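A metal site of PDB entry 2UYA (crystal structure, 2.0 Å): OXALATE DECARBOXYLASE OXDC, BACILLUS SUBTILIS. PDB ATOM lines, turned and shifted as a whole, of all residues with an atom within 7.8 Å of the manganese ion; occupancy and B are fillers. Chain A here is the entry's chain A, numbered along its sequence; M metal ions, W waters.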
ATOM      1  N   VAL A 260     -14.834 -22.427   9.934  1.00  0.00           N
ATOM      2  CA  VAL A 260     -13.721 -21.612  10.341  1.00  0.00           C
ATOM      3  C   VAL A 260     -12.502 -22.487  10.702  1.00  0.00           C
ATOM      4  O   VAL A 260     -12.631 -23.461  11.447  1.00  0.00           O
ATOM      5  CB  VAL A 260     -14.102 -20.741  11.561  1.00  0.00           C
ATOM      6  CG1 VAL A 260     -12.929 -19.777  11.943  1.00  0.00           C
ATOM      7  CG2 VAL A 260     -15.444 -19.974  11.311  1.00  0.00           C
ATOM      8  N   ARG A 268     -10.292 -16.458  16.176  1.00  0.00           N
ATOM      9  CA  ARG A 268     -11.440 -15.804  15.563  1.00  0.00           C
ATOM     10  C   ARG A 268     -11.605 -14.517  16.375  1.00  0.00           C
ATOM     11  O   ARG A 268     -11.757 -14.563  17.594  1.00  0.00           O
ATOM     12  CB  ARG A 268     -12.669 -16.705  15.651  1.00  0.00           C
ATOM     13  CG  ARG A 268     -13.977 -16.128  15.088  1.00  0.00           C
ATOM     14  CD  ARG A 268     -14.071 -16.273  13.584  1.00  0.00           C
ATOM     15  NE  ARG A 268     -15.362 -15.790  13.110  1.00  0.00           N
ATOM     16  CZ  ARG A 268     -15.650 -14.502  12.911  1.00  0.00           C
ATOM     17  NH1 ARG A 268     -14.756 -13.537  13.088  1.00  0.00           N
ATOM     18  NH2 ARG A 268     -16.868 -14.163  12.533  1.00  0.00           N
ATOM     19  N   GLU A 269     -11.521 -13.374  15.698  1.00  0.00           N
ATOM     20  CA  GLU A 269     -11.515 -12.068  16.336  1.00  0.00           C
ATOM     21  C   GLU A 269     -12.777 -11.758  17.162  1.00  0.00           C
ATOM     22  O   GLU A 269     -13.806 -12.420  17.026  1.00  0.00           O
ATOM     23  CB  GLU A 269     -11.293 -10.973  15.263  1.00  0.00           C
ATOM     24  CG  GLU A 269     -12.529 -10.668  14.399  1.00  0.00           C
ATOM     25  CD  GLU A 269     -12.404  -9.406  13.565  1.00  0.00           C
ATOM     26  OE1 GLU A 269     -11.525  -8.555  13.862  1.00  0.00           O
ATOM     27  OE2 GLU A 269     -13.208  -9.272  12.613  1.00  0.00           O
ATOM     28  N   HIS A 271     -16.065 -10.238  17.930  1.00  0.00           N
ATOM     29  CA  HIS A 271     -17.169  -9.915  17.022  1.00  0.00           C
ATOM     30  C   HIS A 271     -18.501 -10.260  17.661  1.00  0.00           C
ATOM     31  O   HIS A 271     -18.550 -10.872  18.745  1.00  0.00           O
ATOM     32  CB  HIS A 271     -16.995 -10.626  15.674  1.00  0.00           C
ATOM     33  CG  HIS A 271     -17.209 -12.097  15.734  1.00  0.00           C
ATOM     34  ND1 HIS A 271     -16.315 -12.960  16.335  1.00  0.00           N
ATOM     35  CD2 HIS A 271     -18.242 -12.865  15.294  1.00  0.00           C
ATOM     36  CE1 HIS A 271     -16.762 -14.190  16.245  1.00  0.00           C
ATOM     37  NE2 HIS A 271     -17.938 -14.153  15.646  1.00  0.00           N
ATOM     38  N   TRP A 272     -19.581  -9.887  17.000  1.00  0.00           N
ATOM     39  CA  TRP A 272     -20.898 -10.439  17.304  1.00  0.00           C
ATOM     40  C   TRP A 272     -21.687 -10.607  16.018  1.00  0.00           C
ATOM     41  O   TRP A 272     -21.269 -10.148  14.956  1.00  0.00           O
ATOM     42  CB  TRP A 272     -21.659  -9.570  18.330  1.00  0.00           C
ATOM     43  CG  TRP A 272     -22.191  -8.261  17.842  1.00  0.00           C
ATOM     44  CD1 TRP A 272     -23.431  -8.029  17.296  1.00  0.00           C
ATOM     45  CD2 TRP A 272     -21.532  -6.988  17.881  1.00  0.00           C
ATOM     46  NE1 TRP A 272     -23.574  -6.705  16.966  1.00  0.00           N
ATOM     47  CE2 TRP A 272     -22.429  -6.033  17.343  1.00  0.00           C
ATOM     48  CE3 TRP A 272     -20.263  -6.564  18.318  1.00  0.00           C
ATOM     49  CZ2 TRP A 272     -22.102  -4.677  17.236  1.00  0.00           C
ATOM     50  CZ3 TRP A 272     -19.935  -5.229  18.205  1.00  0.00           C
ATOM     51  CH2 TRP A 272     -20.852  -4.292  17.677  1.00  0.00           C
ATOM     52  N   HIS A 273     -22.848 -11.268  16.135  1.00  0.00           N
ATOM     53  CA  HIS A 273     -23.769 -11.463  15.029  1.00  0.00           C
ATOM     54  C   HIS A 273     -25.008 -10.666  15.291  1.00  0.00           C
ATOM     55  O   HIS A 273     -25.653 -10.832  16.352  1.00  0.00           O
ATOM     56  CB  HIS A 273     -24.066 -12.943  14.865  1.00  0.00           C
ATOM     57  CG  HIS A 273     -22.819 -13.720  14.632  1.00  0.00           C
ATOM     58  ND1 HIS A 273     -22.147 -13.697  13.433  1.00  0.00           N
ATOM     59  CD2 HIS A 273     -22.072 -14.452  15.471  1.00  0.00           C
ATOM     60  CE1 HIS A 273     -21.051 -14.410  13.545  1.00  0.00           C
ATOM     61  NE2 HIS A 273     -20.976 -14.889  14.763  1.00  0.00           N
ATOM     62  N   GLU A 278     -25.905 -18.051  17.458  1.00  0.00           N
ATOM     63  CA  GLU A 278     -24.910 -18.906  16.816  1.00  0.00           C
ATOM     64  C   GLU A 278     -24.864 -20.236  17.543  1.00  0.00           C
ATOM     65  O   GLU A 278     -24.743 -20.268  18.768  1.00  0.00           O
ATOM     66  CB  GLU A 278     -23.508 -18.278  16.908  1.00  0.00           C
ATOM     67  CG  GLU A 278     -22.364 -19.164  16.318  1.00  0.00           C
ATOM     68  CD  GLU A 278     -20.994 -18.468  16.394  1.00  0.00           C
ATOM     69  OE1 GLU A 278     -20.963 -17.254  16.191  1.00  0.00           O
ATOM     70  OE2 GLU A 278     -19.965 -19.122  16.661  1.00  0.00           O
ATOM     71  N   TRP A 279     -24.912 -21.316  16.779  1.00  0.00           N
ATOM     72  CA  TRP A 279     -24.721 -22.667  17.259  1.00  0.00           C
ATOM     73  C   TRP A 279     -23.376 -23.132  16.655  1.00  0.00           C
ATOM     74  O   TRP A 279     -23.063 -22.809  15.496  1.00  0.00           O
ATOM     75  CB  TRP A 279     -25.893 -23.521  16.785  1.00  0.00           C
ATOM     76  CG  TRP A 279     -25.936 -24.948  17.225  1.00  0.00           C
ATOM     77  CD1 TRP A 279     -26.644 -25.460  18.254  1.00  0.00           C
ATOM     78  CD2 TRP A 279     -25.215 -26.048  16.651  1.00  0.00           C
ATOM     79  NE1 TRP A 279     -26.458 -26.810  18.348  1.00  0.00           N
ATOM     80  CE2 TRP A 279     -25.559 -27.194  17.393  1.00  0.00           C
ATOM     81  CE3 TRP A 279     -24.330 -26.168  15.588  1.00  0.00           C
ATOM     82  CZ2 TRP A 279     -25.038 -28.455  17.111  1.00  0.00           C
ATOM     83  CZ3 TRP A 279     -23.830 -27.450  15.295  1.00  0.00           C
ATOM     84  CH2 TRP A 279     -24.177 -28.557  16.059  1.00  0.00           C
ATOM     85  N   GLN A 280     -22.568 -23.805  17.484  1.00  0.00           N
ATOM     86  CA  GLN A 280     -21.208 -24.194  17.102  1.00  0.00           C
ATOM     87  C   GLN A 280     -21.014 -25.667  17.200  1.00  0.00           C
ATOM     88  O   GLN A 280     -21.551 -26.272  18.125  1.00  0.00           O
ATOM     89  CB  GLN A 280     -20.157 -23.533  18.024  1.00  0.00           C
ATOM     90  CG  GLN A 280     -20.274 -22.017  18.160  1.00  0.00           C
ATOM     91  CD  GLN A 280     -19.255 -21.461  19.170  1.00  0.00           C
ATOM     92  OE1 GLN A 280     -18.906 -22.131  20.155  1.00  0.00           O
ATOM     93  NE2 GLN A 280     -18.786 -20.238  18.919  1.00  0.00           N
ATOM     94  N   MET A 289     -13.610 -19.687  24.501  1.00  0.00           N
ATOM     95  CA  MET A 289     -14.437 -18.576  24.050  1.00  0.00           C
ATOM     96  C   MET A 289     -15.014 -17.907  25.292  1.00  0.00           C
ATOM     97  O   MET A 289     -15.537 -18.606  26.146  1.00  0.00           O
ATOM     98  CB  MET A 289     -15.601 -19.075  23.201  1.00  0.00           C
ATOM     99  CG  MET A 289     -16.696 -18.063  22.995  1.00  0.00           C
ATOM    100  SD  MET A 289     -17.967 -18.515  21.787  1.00  0.00           S
ATOM    101  CE  MET A 289     -18.883 -19.775  22.720  1.00  0.00           C
ATOM    102  N   VAL A 311     -23.842 -19.255  21.139  1.00  0.00           N
ATOM    103  CA  VAL A 311     -23.690 -17.834  21.458  1.00  0.00           C
ATOM    104  C   VAL A 311     -25.035 -17.169  21.173  1.00  0.00           C
ATOM    105  O   VAL A 311     -25.399 -16.988  20.024  1.00  0.00           O
ATOM    106  CB  VAL A 311     -22.623 -17.109  20.625  1.00  0.00           C
ATOM    107  CG1 VAL A 311     -22.435 -15.641  21.128  1.00  0.00           C
ATOM    108  CG2 VAL A 311     -21.278 -17.870  20.609  1.00  0.00           C
ATOM    109  N   MET A 315     -24.536 -11.501  21.436  1.00  0.00           N
ATOM    110  CA  MET A 315     -23.546 -11.514  22.487  1.00  0.00           C
ATOM    111  C   MET A 315     -22.115 -11.449  21.873  1.00  0.00           C
ATOM    112  O   MET A 315     -21.840 -12.037  20.822  1.00  0.00           O
ATOM    113  CB  MET A 315     -23.710 -12.733  23.402  1.00  0.00           C
ATOM    114  CG  MET A 315     -24.993 -12.679  24.214  1.00  0.00           C
ATOM    115  SD  MET A 315     -25.009 -13.857  25.514  1.00  0.00           S
ATOM    116  CE  MET A 315     -26.597 -13.419  26.307  1.00  0.00           C
ATOM    117  N   GLY A 316     -21.245 -10.722  22.556  1.00  0.00           N
ATOM    118  CA  GLY A 316     -19.877 -10.495  22.101  1.00  0.00           C
ATOM    119  C   GLY A 316     -19.085 -11.746  22.338  1.00  0.00           C
ATOM    120  O   GLY A 316     -19.291 -12.417  23.339  1.00  0.00           O
ATOM    121  N   HIS A 317     -18.205 -12.098  21.410  1.00  0.00           N
ATOM    122  CA  HIS A 317     -17.377 -13.277  21.604  1.00  0.00           C
ATOM    123  C   HIS A 317     -16.143 -13.303  20.694  1.00  0.00           C
ATOM    124  O   HIS A 317     -15.950 -12.461  19.832  1.00  0.00           O
ATOM    125  CB  HIS A 317     -18.228 -14.547  21.431  1.00  0.00           C
ATOM    126  CG  HIS A 317     -18.875 -14.653  20.097  1.00  0.00           C
ATOM    127  ND1 HIS A 317     -19.889 -13.816  19.689  1.00  0.00           N
ATOM    128  CD2 HIS A 317     -18.644 -15.495  19.082  1.00  0.00           C
ATOM    129  CE1 HIS A 317     -20.263 -14.152  18.463  1.00  0.00           C
ATOM    130  NE2 HIS A 317     -19.510 -15.168  18.073  1.00  0.00           N
ATOM    131  N   TYR A 318     -15.265 -14.249  21.007  1.00  0.00           N
ATOM    132  CA  TYR A 318     -14.042 -14.521  20.218  1.00  0.00           C
ATOM    133  C   TYR A 318     -13.846 -16.054  20.371  1.00  0.00           C
ATOM    134  O   TYR A 318     -14.381 -16.653  21.309  1.00  0.00           O
ATOM    135  CB  TYR A 318     -12.808 -13.763  20.769  1.00  0.00           C
ATOM    136  CG  TYR A 318     -12.418 -14.244  22.125  1.00  0.00           C
ATOM    137  CD1 TYR A 318     -11.552 -15.320  22.285  1.00  0.00           C
ATOM    138  CD2 TYR A 318     -12.960 -13.673  23.256  1.00  0.00           C
ATOM    139  CE1 TYR A 318     -11.248 -15.801  23.569  1.00  0.00           C
ATOM    140  CE2 TYR A 318     -12.652 -14.127  24.497  1.00  0.00           C
ATOM    141  CZ  TYR A 318     -11.805 -15.197  24.666  1.00  0.00           C
ATOM    142  OH  TYR A 318     -11.527 -15.661  25.962  1.00  0.00           O
ATOM    143  N   VAL A 319     -13.071 -16.670  19.486  1.00  0.00           N
ATOM    144  CA  VAL A 319     -12.719 -18.106  19.659  1.00  0.00           C
ATOM    145  C   VAL A 319     -11.204 -18.267  19.491  1.00  0.00           C
ATOM    146  O   VAL A 319     -10.686 -18.114  18.401  1.00  0.00           O
ATOM    147  CB  VAL A 319     -13.528 -19.052  18.733  1.00  0.00           C
ATOM    148  CG1 VAL A 319     -13.339 -20.485  19.133  1.00  0.00           C
ATOM    149  CG2 VAL A 319     -15.017 -18.715  18.708  1.00  0.00           C
ATOM    150  N   PHE A 329     -13.957 -25.387  13.310  1.00  0.00           N
ATOM    151  CA  PHE A 329     -15.316 -25.399  13.860  1.00  0.00           C
ATOM    152  C   PHE A 329     -16.309 -24.778  12.881  1.00  0.00           C
ATOM    153  O   PHE A 329     -15.945 -24.049  11.962  1.00  0.00           O
ATOM    154  CB  PHE A 329     -15.388 -24.727  15.248  1.00  0.00           C
ATOM    155  CG  PHE A 329     -15.113 -23.239  15.249  1.00  0.00           C
ATOM    156  CD1 PHE A 329     -16.155 -22.315  15.164  1.00  0.00           C
ATOM    157  CD2 PHE A 329     -13.815 -22.750  15.446  1.00  0.00           C
ATOM    158  CE1 PHE A 329     -15.899 -20.959  15.161  1.00  0.00           C
ATOM    159  CE2 PHE A 329     -13.539 -21.375  15.463  1.00  0.00           C
ATOM    160  CZ  PHE A 329     -14.580 -20.479  15.305  1.00  0.00           C
ATOM    161  N   GLU A 331     -19.875 -22.451  12.542  1.00  0.00           N
ATOM    162  CA  GLU A 331     -20.798 -21.453  13.074  1.00  0.00           C
ATOM    163  C   GLU A 331     -22.083 -21.572  12.263  1.00  0.00           C
ATOM    164  O   GLU A 331     -22.049 -21.400  11.040  1.00  0.00           O
ATOM    165  CB  GLU A 331     -20.246 -20.008  12.848  1.00  0.00           C
ATOM    166  CG  GLU A 331     -18.848 -19.723  13.394  1.00  0.00           C
ATOM    167  CD  GLU A 331     -18.278 -18.326  12.984  1.00  0.00           C
ATOM    168  OE1 GLU A 331     -18.658 -17.777  11.900  1.00  0.00           O
ATOM    169  OE2 GLU A 331     -17.414 -17.793  13.741  1.00  0.00           O
ATOM    170  N   ILE A 332     -23.198 -21.877  12.936  1.00  0.00           N
ATOM    171  CA  ILE A 332     -24.493 -22.164  12.314  1.00  0.00           C
ATOM    172  C   ILE A 332     -25.534 -21.160  12.846  1.00  0.00           C
ATOM    173  O   ILE A 332     -25.563 -20.878  14.049  1.00  0.00           O
ATOM    174  CB  ILE A 332     -24.960 -23.633  12.613  1.00  0.00           C
ATOM    175  CG1 ILE A 332     -23.906 -24.648  12.176  1.00  0.00           C
ATOM    176  CG2 ILE A 332     -26.291 -23.903  11.989  1.00  0.00           C
ATOM    177  CD1 ILE A 332     -23.523 -24.652  10.686  1.00  0.00           C
ATOM    178  N   PHE A 333     -26.370 -20.621  11.946  1.00  0.00           N
ATOM    179  CA  PHE A 333     -27.399 -19.611  12.257  1.00  0.00           C
ATOM    180  C   PHE A 333     -28.726 -19.988  11.630  1.00  0.00           C
ATOM    181  O   PHE A 333     -28.742 -20.427  10.485  1.00  0.00           O
ATOM    182  CB  PHE A 333     -26.974 -18.224  11.750  1.00  0.00           C
ATOM    183  CG  PHE A 333     -25.602 -17.841  12.173  1.00  0.00           C
ATOM    184  CD1 PHE A 333     -25.396 -17.093  13.331  1.00  0.00           C
ATOM    185  CD2 PHE A 333     -24.507 -18.259  11.450  1.00  0.00           C
ATOM    186  CE1 PHE A 333     -24.096 -16.815  13.747  1.00  0.00           C
ATOM    187  CE2 PHE A 333     -23.218 -17.979  11.875  1.00  0.00           C
ATOM    188  CZ  PHE A 333     -23.031 -17.250  13.012  1.00  0.00           C
ATOM    189  N   TYR A 338     -25.658 -14.933   6.638  1.00  0.00           N
ATOM    190  CA  TYR A 338     -24.592 -14.820   7.586  1.00  0.00           C
ATOM    191  C   TYR A 338     -24.264 -13.322   7.730  1.00  0.00           C
ATOM    192  O   TYR A 338     -24.208 -12.595   6.728  1.00  0.00           O
ATOM    193  CB  TYR A 338     -23.358 -15.558   7.052  1.00  0.00           C
ATOM    194  CG  TYR A 338     -22.201 -15.441   7.976  1.00  0.00           C
ATOM    195  CD1 TYR A 338     -21.974 -16.393   8.950  1.00  0.00           C
ATOM    196  CD2 TYR A 338     -21.344 -14.342   7.933  1.00  0.00           C
ATOM    197  CE1 TYR A 338     -20.937 -16.276   9.840  1.00  0.00           C
ATOM    198  CE2 TYR A 338     -20.309 -14.229   8.831  1.00  0.00           C
ATOM    199  CZ  TYR A 338     -20.104 -15.204   9.772  1.00  0.00           C
ATOM    200  OH  TYR A 338     -19.077 -15.129  10.688  1.00  0.00           O
ATOM    201  N   ALA A 339     -24.055 -12.867   8.962  1.00  0.00           N
ATOM    202  CA  ALA A 339     -23.647 -11.474   9.184  1.00  0.00           C
ATOM    203  C   ALA A 339     -22.842 -11.415  10.458  1.00  0.00           C
ATOM    204  O   ALA A 339     -23.163 -12.143  11.440  1.00  0.00           O
ATOM    205  CB  ALA A 339     -24.873 -10.546   9.289  1.00  0.00           C
ATOM    206  N   ASP A 340     -21.787 -10.615  10.463  1.00  0.00           N
ATOM    207  CA  ASP A 340     -21.044 -10.317  11.686  1.00  0.00           C
ATOM    208  C   ASP A 340     -20.634  -8.822  11.716  1.00  0.00           C
ATOM    209  O   ASP A 340     -20.559  -8.150  10.689  1.00  0.00           O
ATOM    210  CB  ASP A 340     -19.869 -11.301  11.906  1.00  0.00           C
ATOM    211  CG  ASP A 340     -18.691 -11.125  10.913  1.00  0.00           C
ATOM    212  OD1 ASP A 340     -18.862 -10.558   9.812  1.00  0.00           O
ATOM    213  OD2 ASP A 340     -17.584 -11.590  11.205  1.00  0.00           O
HETATM  214 MN    MN M   1     -19.415 -15.933  15.909  1.00  0.00          MN
HETATM  215  O   HOH W   1     -17.878 -17.476  16.198  1.00  0.00           O
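Water W1 bridges the side-chain carboxylate of Glu 331 (2.5 Å) and the side-chain carboxylate of Glu 278 (2.7 Å).
The side-chain carboxylate (OE2) of Glu 278 lies within hydrogen-bond range of the side-chain amide nitrogen (NE2) of Gln 280, 2.8 Å away. N of Val 311 sits at hydrogen-bond distance from O of Glu 278, at 2.7 Å. ND1 of His 273 sits at hydrogen-bond distance from O of Ala 339 (2.7 Å). O of Met 315 sits at hydrogen-bond distance from ND1 of His 317 (2.9 Å). A ring nitrogen (NE2) of His 271 lies close to the guanidinium group (NH2) of Arg 268, 3.3 Å away. ND1 of His 271 is in hydrogen-bond range of O of Glu 269. The side-chain carboxylate (OE2) of Glu 331 is in salt-bridge range of the guanidinium group (NE) of Arg 268. The side-chain hydroxyl of Tyr 338 lies within hydrogen-bond range of the side-chain carboxylate of Glu 331, 2.9 Å away.
The manganese ion is bound by OE1 of Glu 278 (2.1 Å). Water W1 binds the manganese ion. The manganese ion is bound by a ring nitrogen (NE2) of His 273, at 2.2 Å. NE2 of His 317 binds the manganese ion (2.3 Å). The manganese ion is bound by NE2 of His 271.
Merely in contact with the manganese ion: Glu 331 (3.5 Å). Five residues have an atom within 4 Å of the manganese ion: His 271, His 273, Glu 278, His 317 and Glu 331. Along chain A the residues within 4 Å of the manganese ion span positions 271 to 331. The nearest printed residue that does not touch the manganese ion is Arg 268 (4.6 Å).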
